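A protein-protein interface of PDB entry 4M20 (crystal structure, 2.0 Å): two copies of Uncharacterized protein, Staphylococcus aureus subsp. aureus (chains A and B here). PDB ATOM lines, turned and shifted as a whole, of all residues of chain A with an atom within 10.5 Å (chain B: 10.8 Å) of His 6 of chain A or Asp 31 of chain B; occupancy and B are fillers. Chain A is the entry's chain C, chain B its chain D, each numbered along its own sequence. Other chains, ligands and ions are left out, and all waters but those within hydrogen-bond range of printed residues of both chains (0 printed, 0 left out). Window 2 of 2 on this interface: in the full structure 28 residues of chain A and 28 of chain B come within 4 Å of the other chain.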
ATOM      1  N   HIS A   6      12.877 -21.850  -2.834  1.00  0.00           N
ATOM      2  CA  HIS A   6      12.150 -22.521  -3.905  1.00  0.00           C
ATOM      3  C   HIS A   6      11.905 -24.012  -3.610  1.00  0.00           C
ATOM      4  O   HIS A   6      10.880 -24.565  -4.025  1.00  0.00           O
ATOM      5  CB  HIS A   6      12.900 -22.363  -5.227  1.00  0.00           C
ATOM      6  CG  HIS A   6      12.014 -22.035  -6.390  1.00  0.00           C
ATOM      7  ND1 HIS A   6      12.331 -21.065  -7.316  1.00  0.00           N
ATOM      8  CD2 HIS A   6      10.820 -22.546  -6.777  1.00  0.00           C
ATOM      9  CE1 HIS A   6      11.371 -20.990  -8.221  1.00  0.00           C
ATOM     10  NE2 HIS A   6      10.442 -21.880  -7.918  1.00  0.00           N
ATOM     11  N   LEU A   7      12.831 -24.666  -2.905  1.00  0.00           N
ATOM     12  CA  LEU A   7      12.562 -26.018  -2.418  1.00  0.00           C
ATOM     13  C   LEU A   7      11.407 -25.974  -1.430  1.00  0.00           C
ATOM     14  O   LEU A   7      10.563 -26.875  -1.395  1.00  0.00           O
ATOM     15  CB  LEU A   7      13.781 -26.644  -1.737  1.00  0.00           C
ATOM     16  CG  LEU A   7      13.439 -28.029  -1.155  1.00  0.00           C
ATOM     17  CD1 LEU A   7      13.150 -29.044  -2.245  1.00  0.00           C
ATOM     18  CD2 LEU A   7      14.488 -28.544  -0.211  1.00  0.00           C
ATOM     19  N   LEU A   8      11.367 -24.902  -0.645  1.00  0.00           N
ATOM     20  CA  LEU A   8      10.285 -24.676   0.300  1.00  0.00           C
ATOM     21  C   LEU A   8       8.949 -24.715  -0.409  1.00  0.00           C
ATOM     22  O   LEU A   8       7.976 -25.249   0.118  1.00  0.00           O
ATOM     23  CB  LEU A   8      10.447 -23.333   1.012  1.00  0.00           C
ATOM     24  CG  LEU A   8      11.563 -23.166   2.045  1.00  0.00           C
ATOM     25  CD1 LEU A   8      12.955 -23.013   1.413  1.00  0.00           C
ATOM     26  CD2 LEU A   8      11.227 -21.984   2.941  1.00  0.00           C
ATOM     27  N   GLU A   9       8.906 -24.122  -1.601  1.00  0.00           N
ATOM     28  CA  GLU A   9       7.707 -24.152  -2.424  1.00  0.00           C
ATOM     29  C   GLU A   9       7.541 -25.527  -3.049  1.00  0.00           C
ATOM     30  O   GLU A   9       6.428 -26.050  -3.121  1.00  0.00           O
ATOM     31  CB  GLU A   9       7.747 -23.064  -3.509  1.00  0.00           C
ATOM     32  CG  GLU A   9       7.128 -21.735  -3.069  1.00  0.00           C
ATOM     33  CD  GLU A   9       6.991 -20.707  -4.204  1.00  0.00           C
ATOM     34  OE1 GLU A   9       6.883 -21.110  -5.383  1.00  0.00           O
ATOM     35  OE2 GLU A   9       6.994 -19.490  -3.911  1.00  0.00           O
ATOM     36  N   THR A  10       8.643 -26.112  -3.511  1.00  0.00           N
ATOM     37  CA  THR A  10       8.582 -27.444  -4.104  1.00  0.00           C
ATOM     38  C   THR A  10       7.973 -28.432  -3.108  1.00  0.00           C
ATOM     39  O   THR A  10       7.162 -29.279  -3.482  1.00  0.00           O
ATOM     40  CB  THR A  10       9.965 -27.929  -4.546  1.00  0.00           C
ATOM     41  OG1 THR A  10      10.545 -26.964  -5.427  1.00  0.00           O
ATOM     42  CG2 THR A  10       9.860 -29.264  -5.264  1.00  0.00           C
ATOM     43  N   PHE A  11       8.347 -28.293  -1.836  1.00  0.00           N
ATOM     44  CA  PHE A  11       7.845 -29.172  -0.781  1.00  0.00           C
ATOM     45  C   PHE A  11       6.592 -28.619  -0.124  1.00  0.00           C
ATOM     46  O   PHE A  11       6.050 -29.228   0.797  1.00  0.00           O
ATOM     47  CB  PHE A  11       8.903 -29.413   0.301  1.00  0.00           C
ATOM     48  CG  PHE A  11       9.951 -30.408  -0.091  1.00  0.00           C
ATOM     49  CD1 PHE A  11      10.012 -30.892  -1.387  1.00  0.00           C
ATOM     50  CD2 PHE A  11      10.815 -30.927   0.852  1.00  0.00           C
ATOM     51  CE1 PHE A  11      10.959 -31.817  -1.752  1.00  0.00           C
ATOM     52  CE2 PHE A  11      11.757 -31.858   0.491  1.00  0.00           C
ATOM     53  CZ  PHE A  11      11.829 -32.304  -0.813  1.00  0.00           C
ATOM     54  N   GLU A  12       6.143 -27.464  -0.602  1.00  0.00           N
ATOM     55  CA  GLU A  12       4.930 -26.823  -0.103  1.00  0.00           C
ATOM     56  C   GLU A  12       5.014 -26.570   1.396  1.00  0.00           C
ATOM     57  O   GLU A  12       4.054 -26.820   2.125  1.00  0.00           O
ATOM     58  CB  GLU A  12       3.711 -27.700  -0.436  1.00  0.00           C
ATOM     59  CG  GLU A  12       3.515 -27.882  -1.937  1.00  0.00           C
ATOM     60  CD  GLU A  12       2.335 -28.765  -2.310  1.00  0.00           C
ATOM     61  OE1 GLU A  12       1.632 -29.274  -1.415  1.00  0.00           O
ATOM     62  OE2 GLU A  12       2.133 -28.974  -3.521  1.00  0.00           O
ATOM     63  N   MET A  13       6.163 -26.055   1.844  1.00  0.00           N
ATOM     64  CA  MET A  13       6.398 -25.792   3.262  1.00  0.00           C
ATOM     65  C   MET A  13       5.643 -24.554   3.730  1.00  0.00           C
ATOM     66  O   MET A  13       5.522 -23.578   2.999  1.00  0.00           O
ATOM     67  CB  MET A  13       7.895 -25.614   3.546  1.00  0.00           C
ATOM     68  CG  MET A  13       8.758 -26.787   3.142  1.00  0.00           C
ATOM     69  SD  MET A  13      10.487 -26.545   3.619  1.00  0.00           S
ATOM     70  CE  MET A  13      11.275 -27.904   2.756  1.00  0.00           C
ATOM     71  N   ILE A  15       5.511 -21.873   7.058  1.00  0.00           N
ATOM     72  CA  ILE A  15       6.071 -21.410   8.324  1.00  0.00           C
ATOM     73  C   ILE A  15       4.950 -21.109   9.306  1.00  0.00           C
ATOM     74  O   ILE A  15       4.191 -20.156   9.133  1.00  0.00           O
ATOM     75  CB  ILE A  15       6.957 -20.163   8.159  1.00  0.00           C
ATOM     76  CG1 ILE A  15       8.202 -20.489   7.346  1.00  0.00           C
ATOM     77  CG2 ILE A  15       7.436 -19.691   9.502  1.00  0.00           C
ATOM     78  CD1 ILE A  15       8.061 -20.209   5.881  1.00  0.00           C
ATOM     79  N   LYS A  32       4.942 -36.291  -4.141  1.00  0.00           N
ATOM     80  CA  LYS A  32       6.156 -35.561  -4.527  1.00  0.00           C
ATOM     81  C   LYS A  32       7.347 -35.817  -3.585  1.00  0.00           C
ATOM     82  O   LYS A  32       8.504 -35.719  -4.001  1.00  0.00           O
ATOM     83  CB  LYS A  32       5.887 -34.047  -4.561  1.00  0.00           C
ATOM     84  CG  LYS A  32       5.075 -33.535  -5.746  1.00  0.00           C
ATOM     85  CD  LYS A  32       4.751 -32.040  -5.600  1.00  0.00           C
ATOM     86  CE  LYS A  32       5.819 -31.134  -6.214  1.00  0.00           C
ATOM     87  NZ  LYS A  32       5.410 -29.694  -6.152  1.00  0.00           N
ATOM     88  N   VAL A  33       7.066 -36.179  -2.336  1.00  0.00           N
ATOM     89  CA  VAL A  33       8.123 -36.375  -1.337  1.00  0.00           C
ATOM     90  C   VAL A  33       8.221 -37.798  -0.758  1.00  0.00           C
ATOM     91  O   VAL A  33       8.810 -37.997   0.306  1.00  0.00           O
ATOM     92  CB  VAL A  33       7.951 -35.374  -0.182  1.00  0.00           C
ATOM     93  CG1 VAL A  33       8.194 -33.943  -0.687  1.00  0.00           C
ATOM     94  CG2 VAL A  33       6.560 -35.492   0.417  1.00  0.00           C
ATOM     95  N   ALA A  47      15.351 -32.575   4.749  1.00  0.00           N
ATOM     96  CA  ALA A  47      15.349 -31.319   4.013  1.00  0.00           C
ATOM     97  C   ALA A  47      14.503 -30.276   4.734  1.00  0.00           C
ATOM     98  O   ALA A  47      14.866 -29.090   4.812  1.00  0.00           O
ATOM     99  CB  ALA A  47      14.845 -31.544   2.573  1.00  0.00           C
ATOM    100  N   THR A  51      15.949 -26.842   6.463  1.00  0.00           N
ATOM    101  CA  THR A  51      15.227 -25.595   6.179  1.00  0.00           C
ATOM    102  C   THR A  51      14.871 -24.861   7.467  1.00  0.00           C
ATOM    103  O   THR A  51      15.084 -23.649   7.601  1.00  0.00           O
ATOM    104  CB  THR A  51      13.919 -25.858   5.372  1.00  0.00           C
ATOM    105  OG1 THR A  51      14.248 -26.531   4.155  1.00  0.00           O
ATOM    106  CG2 THR A  51      13.191 -24.552   5.049  1.00  0.00           C
ATOM    107  N   THR B  10      10.775 -36.263  -8.796  1.00  0.00           N
ATOM    108  CA  THR B  10      10.739 -34.840  -8.478  1.00  0.00           C
ATOM    109  C   THR B  10      12.102 -34.186  -8.694  1.00  0.00           C
ATOM    110  O   THR B  10      12.194 -33.039  -9.123  1.00  0.00           O
ATOM    111  CB  THR B  10      10.311 -34.592  -7.021  1.00  0.00           C
ATOM    112  OG1 THR B  10       9.082 -35.276  -6.748  1.00  0.00           O
ATOM    113  CG2 THR B  10      10.144 -33.104  -6.766  1.00  0.00           C
ATOM    114  N   PHE B  11      13.158 -34.911  -8.346  1.00  0.00           N
ATOM    115  CA  PHE B  11      14.513 -34.392  -8.474  1.00  0.00           C
ATOM    116  C   PHE B  11      15.211 -34.800  -9.792  1.00  0.00           C
ATOM    117  O   PHE B  11      16.352 -34.404 -10.030  1.00  0.00           O
ATOM    118  CB  PHE B  11      15.342 -34.859  -7.276  1.00  0.00           C
ATOM    119  CG  PHE B  11      15.007 -34.149  -5.976  1.00  0.00           C
ATOM    120  CD1 PHE B  11      13.957 -33.251  -5.898  1.00  0.00           C
ATOM    121  CD2 PHE B  11      15.733 -34.408  -4.828  1.00  0.00           C
ATOM    122  CE1 PHE B  11      13.649 -32.619  -4.704  1.00  0.00           C
ATOM    123  CE2 PHE B  11      15.426 -33.782  -3.638  1.00  0.00           C
ATOM    124  CZ  PHE B  11      14.386 -32.887  -3.579  1.00  0.00           C
ATOM    125  N   GLU B  12      14.517 -35.556 -10.649  1.00  0.00           N
ATOM    126  CA  GLU B  12      15.070 -36.044 -11.931  1.00  0.00           C
ATOM    127  C   GLU B  12      16.353 -36.844 -11.776  1.00  0.00           C
ATOM    128  O   GLU B  12      17.342 -36.602 -12.469  1.00  0.00           O
ATOM    129  CB  GLU B  12      15.315 -34.909 -12.943  1.00  0.00           C
ATOM    130  CG  GLU B  12      14.078 -34.278 -13.562  1.00  0.00           C
ATOM    131  CD  GLU B  12      13.447 -33.233 -12.701  1.00  0.00           C
ATOM    132  OE1 GLU B  12      13.813 -33.128 -11.519  1.00  0.00           O
ATOM    133  OE2 GLU B  12      12.575 -32.500 -13.207  1.00  0.00           O
ATOM    134  N   MET B  27      21.626 -36.045 -10.438  1.00  0.00           N
ATOM    135  CA  MET B  27      20.423 -35.232 -10.610  1.00  0.00           C
ATOM    136  C   MET B  27      20.832 -33.830 -11.026  1.00  0.00           C
ATOM    137  O   MET B  27      21.937 -33.380 -10.709  1.00  0.00           O
ATOM    138  CB  MET B  27      19.569 -35.154  -9.345  1.00  0.00           C
ATOM    139  CG  MET B  27      20.144 -34.246  -8.275  1.00  0.00           C
ATOM    140  SD  MET B  27      19.119 -34.040  -6.797  1.00  0.00           S
ATOM    141  CE  MET B  27      18.696 -35.718  -6.436  1.00  0.00           C
ATOM    142  N   PRO B  28      19.948 -33.135 -11.755  1.00  0.00           N
ATOM    143  CA  PRO B  28      20.254 -31.767 -12.168  1.00  0.00           C
ATOM    144  C   PRO B  28      20.031 -30.789 -11.030  1.00  0.00           C
ATOM    145  O   PRO B  28      19.101 -30.962 -10.242  1.00  0.00           O
ATOM    146  CB  PRO B  28      19.259 -31.512 -13.297  1.00  0.00           C
ATOM    147  CG  PRO B  28      18.086 -32.345 -12.927  1.00  0.00           C
ATOM    148  CD  PRO B  28      18.647 -33.584 -12.281  1.00  0.00           C
ATOM    149  N   VAL B  29      20.883 -29.777 -10.959  1.00  0.00           N
ATOM    150  CA  VAL B  29      20.736 -28.695  -9.999  1.00  0.00           C
ATOM    151  C   VAL B  29      19.830 -27.633 -10.592  1.00  0.00           C
ATOM    152  O   VAL B  29      20.284 -26.837 -11.391  1.00  0.00           O
ATOM    153  CB  VAL B  29      22.095 -28.049  -9.639  1.00  0.00           C
ATOM    154  CG1 VAL B  29      21.894 -26.895  -8.664  1.00  0.00           C
ATOM    155  CG2 VAL B  29      23.052 -29.079  -9.066  1.00  0.00           C
ATOM    156  N   THR B  30      18.546 -27.648 -10.257  1.00  0.00           N
ATOM    157  CA  THR B  30      17.618 -26.656 -10.803  1.00  0.00           C
ATOM    158  C   THR B  30      16.973 -25.830  -9.686  1.00  0.00           C
ATOM    159  O   THR B  30      17.264 -26.056  -8.514  1.00  0.00           O
ATOM    160  CB  THR B  30      16.544 -27.325 -11.669  1.00  0.00           C
ATOM    161  OG1 THR B  30      15.671 -28.093 -10.841  1.00  0.00           O
ATOM    162  CG2 THR B  30      17.198 -28.253 -12.687  1.00  0.00           C
ATOM    163  N   ASP B  31      16.120 -24.867 -10.040  1.00  0.00           N
ATOM    164  CA  ASP B  31      15.477 -24.017  -9.028  1.00  0.00           C
ATOM    165  C   ASP B  31      14.639 -24.767  -8.000  1.00  0.00           C
ATOM    166  O   ASP B  31      14.599 -24.401  -6.837  1.00  0.00           O
ATOM    167  CB  ASP B  31      14.575 -22.960  -9.679  1.00  0.00           C
ATOM    168  CG  ASP B  31      15.354 -21.813 -10.291  1.00  0.00           C
ATOM    169  OD1 ASP B  31      16.358 -21.382  -9.685  1.00  0.00           O
ATOM    170  OD2 ASP B  31      14.937 -21.306 -11.351  1.00  0.00           O
ATOM    171  N   LYS B  32      13.967 -25.819  -8.426  1.00  0.00           N
ATOM    172  CA  LYS B  32      13.119 -26.587  -7.520  1.00  0.00           C
ATOM    173  C   LYS B  32      13.838 -27.237  -6.327  1.00  0.00           C
ATOM    174  O   LYS B  32      13.197 -27.678  -5.375  1.00  0.00           O
ATOM    175  CB  LYS B  32      12.406 -27.623  -8.335  1.00  0.00           C
ATOM    176  CG  LYS B  32      13.315 -28.664  -8.857  1.00  0.00           C
ATOM    177  CD  LYS B  32      12.540 -29.325  -9.926  1.00  0.00           C
ATOM    178  CE  LYS B  32      13.418 -30.116 -10.835  1.00  0.00           C
ATOM    179  NZ  LYS B  32      12.592 -30.656 -11.957  1.00  0.00           N
ATOM    180  N   VAL B  33      15.155 -27.379  -6.416  1.00  0.00           N
ATOM    181  CA  VAL B  33      15.901 -27.982  -5.324  1.00  0.00           C
ATOM    182  C   VAL B  33      16.864 -26.975  -4.722  1.00  0.00           C
ATOM    183  O   VAL B  33      17.762 -27.349  -3.966  1.00  0.00           O
ATOM    184  CB  VAL B  33      16.689 -29.230  -5.777  1.00  0.00           C
ATOM    185  CG1 VAL B  33      15.737 -30.327  -6.157  1.00  0.00           C
ATOM    186  CG2 VAL B  33      17.601 -28.901  -6.944  1.00  0.00           C
ATOM    187  N   LYS B  34      16.665 -25.697  -5.044  1.00  0.00           N
ATOM    188  CA  LYS B  34      17.535 -24.633  -4.545  1.00  0.00           C
ATOM    189  C   LYS B  34      17.007 -23.946  -3.288  1.00  0.00           C
ATOM    190  O   LYS B  34      15.810 -23.967  -3.005  1.00  0.00           O
ATOM    191  CB  LYS B  34      17.756 -23.564  -5.627  1.00  0.00           C
ATOM    192  CG  LYS B  34      18.769 -23.930  -6.701  1.00  0.00           C
ATOM    193  CD  LYS B  34      18.929 -22.782  -7.678  1.00  0.00           C
ATOM    194  CE  LYS B  34      19.950 -23.089  -8.753  1.00  0.00           C
ATOM    195  NZ  LYS B  34      20.133 -21.922  -9.668  1.00  0.00           N
ATOM    196  N   GLN B  35      17.918 -23.305  -2.559  1.00  0.00           N
ATOM    197  CA  GLN B  35      17.555 -22.378  -1.493  1.00  0.00           C
ATOM    198  C   GLN B  35      17.143 -21.056  -2.108  1.00  0.00           C
ATOM    199  O   GLN B  35      17.313 -20.864  -3.311  1.00  0.00           O
ATOM    200  CB  GLN B  35      18.719 -22.178  -0.509  1.00  0.00           C
ATOM    201  CG  GLN B  35      18.852 -23.229   0.578  1.00  0.00           C
ATOM    202  CD  GLN B  35      17.686 -23.196   1.576  1.00  0.00           C
ATOM    203  OE1 GLN B  35      16.515 -23.284   1.201  1.00  0.00           O
ATOM    204  NE2 GLN B  35      18.016 -23.050   2.858  1.00  0.00           N
ATOM    205  N   PRO B  36      16.542 -20.159  -1.307  1.00  0.00           N
ATOM    206  CA  PRO B  36      16.114 -18.892  -1.907  1.00  0.00           C
ATOM    207  C   PRO B  36      17.265 -18.061  -2.472  1.00  0.00           C
ATOM    208  O   PRO B  36      17.070 -17.425  -3.506  1.00  0.00           O
ATOM    209  CB  PRO B  36      15.444 -18.156  -0.736  1.00  0.00           C
ATOM    210  CG  PRO B  36      15.890 -18.885   0.503  1.00  0.00           C
ATOM    211  CD  PRO B  36      16.037 -20.301   0.069  1.00  0.00           C
ATOM    212  N   PHE B  37      18.432 -18.084  -1.829  1.00  0.00           N
ATOM    213  CA  PHE B  37      19.516 -17.160  -2.176  1.00  0.00           C
ATOM    214  C   PHE B  37      19.931 -17.133  -3.668  1.00  0.00           C
ATOM    215  O   PHE B  37      20.003 -16.040  -4.232  1.00  0.00           O
ATOM    216  CB  PHE B  37      20.758 -17.426  -1.307  1.00  0.00           C
ATOM    217  CG  PHE B  37      21.954 -16.573  -1.673  1.00  0.00           C
ATOM    218  CD1 PHE B  37      22.163 -15.352  -1.049  1.00  0.00           C
ATOM    219  CD2 PHE B  37      22.860 -16.981  -2.640  1.00  0.00           C
ATOM    220  CE1 PHE B  37      23.249 -14.558  -1.377  1.00  0.00           C
ATOM    221  CE2 PHE B  37      23.952 -16.188  -2.974  1.00  0.00           C
ATOM    222  CZ  PHE B  37      24.145 -14.977  -2.339  1.00  0.00           C
ATOM    223  N   GLY B  38      20.200 -18.268  -4.330  1.00  0.00           N
ATOM    224  CA  GLY B  38      20.071 -19.615  -3.808  1.00  0.00           C
ATOM    225  C   GLY B  38      21.023 -20.638  -4.405  1.00  0.00           C
ATOM    226  O   GLY B  38      21.288 -20.671  -5.610  1.00  0.00           O
ATOM    227  N   TYR B  39      21.526 -21.500  -3.529  1.00  0.00           N
ATOM    228  CA  TYR B  39      22.404 -22.589  -3.914  1.00  0.00           C
ATOM    229  C   TYR B  39      21.618 -23.900  -3.948  1.00  0.00           C
ATOM    230  O   TYR B  39      20.432 -23.924  -3.631  1.00  0.00           O
ATOM    231  CB  TYR B  39      23.548 -22.708  -2.906  1.00  0.00           C
ATOM    232  CG  TYR B  39      24.388 -21.464  -2.746  1.00  0.00           C
ATOM    233  CD1 TYR B  39      25.542 -21.278  -3.488  1.00  0.00           C
ATOM    234  CD2 TYR B  39      24.031 -20.478  -1.833  1.00  0.00           C
ATOM    235  CE1 TYR B  39      26.321 -20.146  -3.328  1.00  0.00           C
ATOM    236  CE2 TYR B  39      24.805 -19.340  -1.669  1.00  0.00           C
ATOM    237  CZ  TYR B  39      25.945 -19.176  -2.426  1.00  0.00           C
ATOM    238  OH  TYR B  39      26.721 -18.050  -2.278  1.00  0.00           O
ATOM    239  N   LEU B  40      22.275 -24.986  -4.338  1.00  0.00           N
ATOM    240  CA  LEU B  40      21.700 -26.302  -4.121  1.00  0.00           C
ATOM    241  C   LEU B  40      21.399 -26.419  -2.629  1.00  0.00           C
ATOM    242  O   LEU B  40      22.256 -26.121  -1.803  1.00  0.00           O
ATOM    243  CB  LEU B  40      22.647 -27.411  -4.577  1.00  0.00           C
ATOM    244  CG  LEU B  40      22.101 -28.817  -4.331  1.00  0.00           C
ATOM    245  CD1 LEU B  40      20.795 -28.978  -5.093  1.00  0.00           C
ATOM    246  CD2 LEU B  40      23.108 -29.911  -4.710  1.00  0.00           C
ATOM    247  N   HIS B  41      20.173 -26.802  -2.294  1.00  0.00           N
ATOM    248  CA  HIS B  41      19.746 -26.972  -0.909  1.00  0.00           C
ATOM    249  C   HIS B  41      20.487 -28.157  -0.295  1.00  0.00           C
ATOM    250  O   HIS B  41      20.604 -29.202  -0.934  1.00  0.00           O
ATOM    251  CB  HIS B  41      18.225 -27.178  -0.864  1.00  0.00           C
ATOM    252  CG  HIS B  41      17.607 -27.043   0.498  1.00  0.00           C
ATOM    253  ND1 HIS B  41      17.871 -27.915   1.532  1.00  0.00           N
ATOM    254  CD2 HIS B  41      16.679 -26.176   0.970  1.00  0.00           C
ATOM    255  CE1 HIS B  41      17.157 -27.576   2.591  1.00  0.00           C
ATOM    256  NE2 HIS B  41      16.421 -26.526   2.274  1.00  0.00           N
ATOM    257  N   GLY B  42      21.016 -27.988   0.917  1.00  0.00           N
ATOM    258  CA  GLY B  42      21.736 -29.065   1.591  1.00  0.00           C
ATOM    259  C   GLY B  42      20.873 -30.310   1.750  1.00  0.00           C
ATOM    260  O   GLY B  42      21.341 -31.453   1.638  1.00  0.00           O
ATOM    261  N   ALA B  44      18.511 -31.280  -0.283  1.00  0.00           N
ATOM    262  CA  ALA B  44      18.296 -31.977  -1.561  1.00  0.00           C
ATOM    263  C   ALA B  44      19.449 -32.919  -1.836  1.00  0.00           C
ATOM    264  O   ALA B  44      19.265 -34.058  -2.265  1.00  0.00           O
ATOM    265  CB  ALA B  44      18.143 -30.986  -2.703  1.00  0.00           C
ATOM    266  N   ALA B  81      26.850 -25.702  -4.693  1.00  0.00           N
ATOM    267  CA  ALA B  81      26.591 -26.013  -6.089  1.00  0.00           C
ATOM    268  C   ALA B  81      25.562 -25.019  -6.590  1.00  0.00           C
ATOM    269  O   ALA B  81      24.526 -24.810  -5.954  1.00  0.00           O
ATOM    270  CB  ALA B  81      26.103 -27.436  -6.255  1.00  0.00           C
ATOM    271  N   LYS B  82      25.850 -24.397  -7.725  1.00  0.00           N
ATOM    272  CA  LYS B  82      24.973 -23.363  -8.238  1.00  0.00           C
ATOM    273  C   LYS B  82      24.241 -23.826  -9.482  1.00  0.00           C
ATOM    274  O   LYS B  82      23.139 -23.357  -9.761  1.00  0.00           O
ATOM    275  CB  LYS B  82      25.777 -22.103  -8.550  1.00  0.00           C
ATOM    276  CG  LYS B  82      26.395 -21.435  -7.343  1.00  0.00           C
ATOM    277  CD  LYS B  82      25.462 -20.385  -6.767  1.00  0.00           C
ATOM    278  CE  LYS B  82      26.224 -19.108  -6.439  1.00  0.00           C
ATOM    279  NZ  LYS B  82      25.331 -18.013  -5.972  1.00  0.00           N
ATOM    280  N   ASP B  83      24.834 -24.771 -10.204  1.00  0.00           N
ATOM    281  CA  ASP B  83      24.260 -25.219 -11.464  1.00  0.00           C
ATOM    282  C   ASP B  83      24.786 -26.574 -11.905  1.00  0.00           C
ATOM    283  O   ASP B  83      25.623 -27.179 -11.242  1.00  0.00           O
ATOM    284  CB  ASP B  83      24.542 -24.194 -12.568  1.00  0.00           C
ATOM    285  CG  ASP B  83      26.027 -24.015 -12.835  1.00  0.00           C
ATOM    286  OD1 ASP B  83      26.846 -24.364 -11.958  1.00  0.00           O
ATOM    287  OD2 ASP B  83      26.380 -23.528 -13.929  1.00  0.00           O
ATOM    288  N   GLY B  84      24.295 -27.035 -13.046  1.00  0.00           N
ATOM    289  CA  GLY B  84      24.725 -28.303 -13.588  1.00  0.00           C
ATOM    290  C   GLY B  84      24.135 -29.495 -12.868  1.00  0.00           C
ATOM    291  O   GLY B  84      22.982 -29.471 -12.436  1.00  0.00           O
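The backbone carbonyl oxygen of Lys 32 of chain A sits at hydrogen-bond distance from the side-chain hydroxyl of Thr 10 of chain B, at 2.8 Å.
The side-chain hydroxyl (OG1) of Thr 10 of chain A is in hydrogen-bond range of the backbone carbonyl oxygen (O) of Lys 32 of chain B, at 2.7 Å.
The side-chain hydroxyl (OG1) of Thr 51 of chain A is in hydrogen-bond range of a ring nitrogen (NE2) of His 41 of chain B.
O of Lys 34 of chain B sits at hydrogen-bond distance from N of Leu 7 of chain A, at 3.1 Å.
SD of Met 13 of chain A lies close to OG1 of Thr 51 of chain A.
The side-chain amino group of Lys 34 of chain B is in hydrogen-bond range of the backbone carbonyl oxygen of Lys 82 of chain B, at 3.3 Å.
The side-chain carboxylate (OE1) of Glu 12 of chain B is in salt-bridge range of the side-chain amino group (NZ) of Lys 32 of chain B, 2.8 Å away.
The backbone carbonyl oxygen (O) of Ala 47 of chain A is in hydrogen-bond range of the side-chain hydroxyl (OG1) of Thr 51 of chain A, 2.7 Å away.
O of Leu 8 of chain A lies within hydrogen-bond range of N of Met 13 of chain A, at 2.6 Å.
The backbone NH (N) of His 41 of chain B lies within hydrogen-bond range of the backbone carbonyl oxygen (O) of Val 33 of chain B (3.0 Å).
Thr 10 of chain A touches Lys 32 of chain B, and with the chains exchanged Lys 32 of chain A touches Thr 10 of chain B.
Phe 11 of chain B touches its own counterpart, Phe 11 of chain A.
Positions printed for both chains: 10, 11, 12, 32 and 33.
Among the printed residues, pairs that only touch across the chains: His 6 of chain A with Asp 31 of chain B (3.1 Å), Leu 7 of chain A with Lys 32 of chain B (3.4 Å), Leu 7 of chain A with His 41 of chain B (3.4 Å), Ala 47 of chain A with His 41 of chain B (3.5 Å), Leu 8 of chain A with Gln 35 of chain B (3.6 Å), His 6 of chain A with Lys 34 of chain B (3.6 Å) and Phe 11 of chain A with Phe 11 of chain B (3.8 Å).
His 6 of chain A touches just these residues of chain B: Asp 31 and Lys 34.
Leu 7 of chain A touches just these residues of chain B: Lys 32, Lys 34 and His 41.
No residue of chain B comes within 4 Å of Glu 9 of chain A.
Of chain B, only Lys 32 (2.7 Å) comes within 4 Å of Thr 10 of chain A.
Of the printed residues of chain B, Lys 32 of chain A touches Thr 10.
Printed residues of chain B within 4 Å of Thr 51 of chain A: His 41.
Printed residues of chain A within 4 Å of Phe 11 of chain B: Phe 11 (3.8 Å).
No residue of chain A comes within 4 Å of Thr 30 of chain B.
Asp 31 of chain B touches one residue of chain A.
Of the printed residues of chain A, Lys 32 of chain B touches Leu 7 and Thr 10.
No residue of chain A comes within 4 Å of Val 33 of chain B.
Lys 34 of chain B touches just these residues of chain A: His 6 and Leu 7.
Of the printed residues of chain A, Gln 35 of chain B touches Leu 8 (3.6 Å).
The nearest residue of chain B that does not touch His 6 of chain A is Lys 32 of chain B (4.1 Å).
The nearest printed residue of chain B that does not touch Phe 11 of chain A is Thr 10 of chain B (5.2 Å).
Of the 24 printed residues of chain B, 7 touch a printed residue of chain A.
Along chain B the printed residues that touch a printed residue of chain A span positions 10 to 41.
Printed residues of chain A that touch a printed residue of chain B: His 6, Leu 7, Leu 8, Thr 10, Phe 11, Lys 32, Ala 47 and Thr 51.
Hydrophobic or aromatic side chains of chain A that line the printed part of chain B: His 6, Leu 7, Leu 8 and Phe 11.
Among the printed residues, no Asp or Glu carboxylate lies within 4 Å of a Lys or Arg side-chain nitrogen of the other chain.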
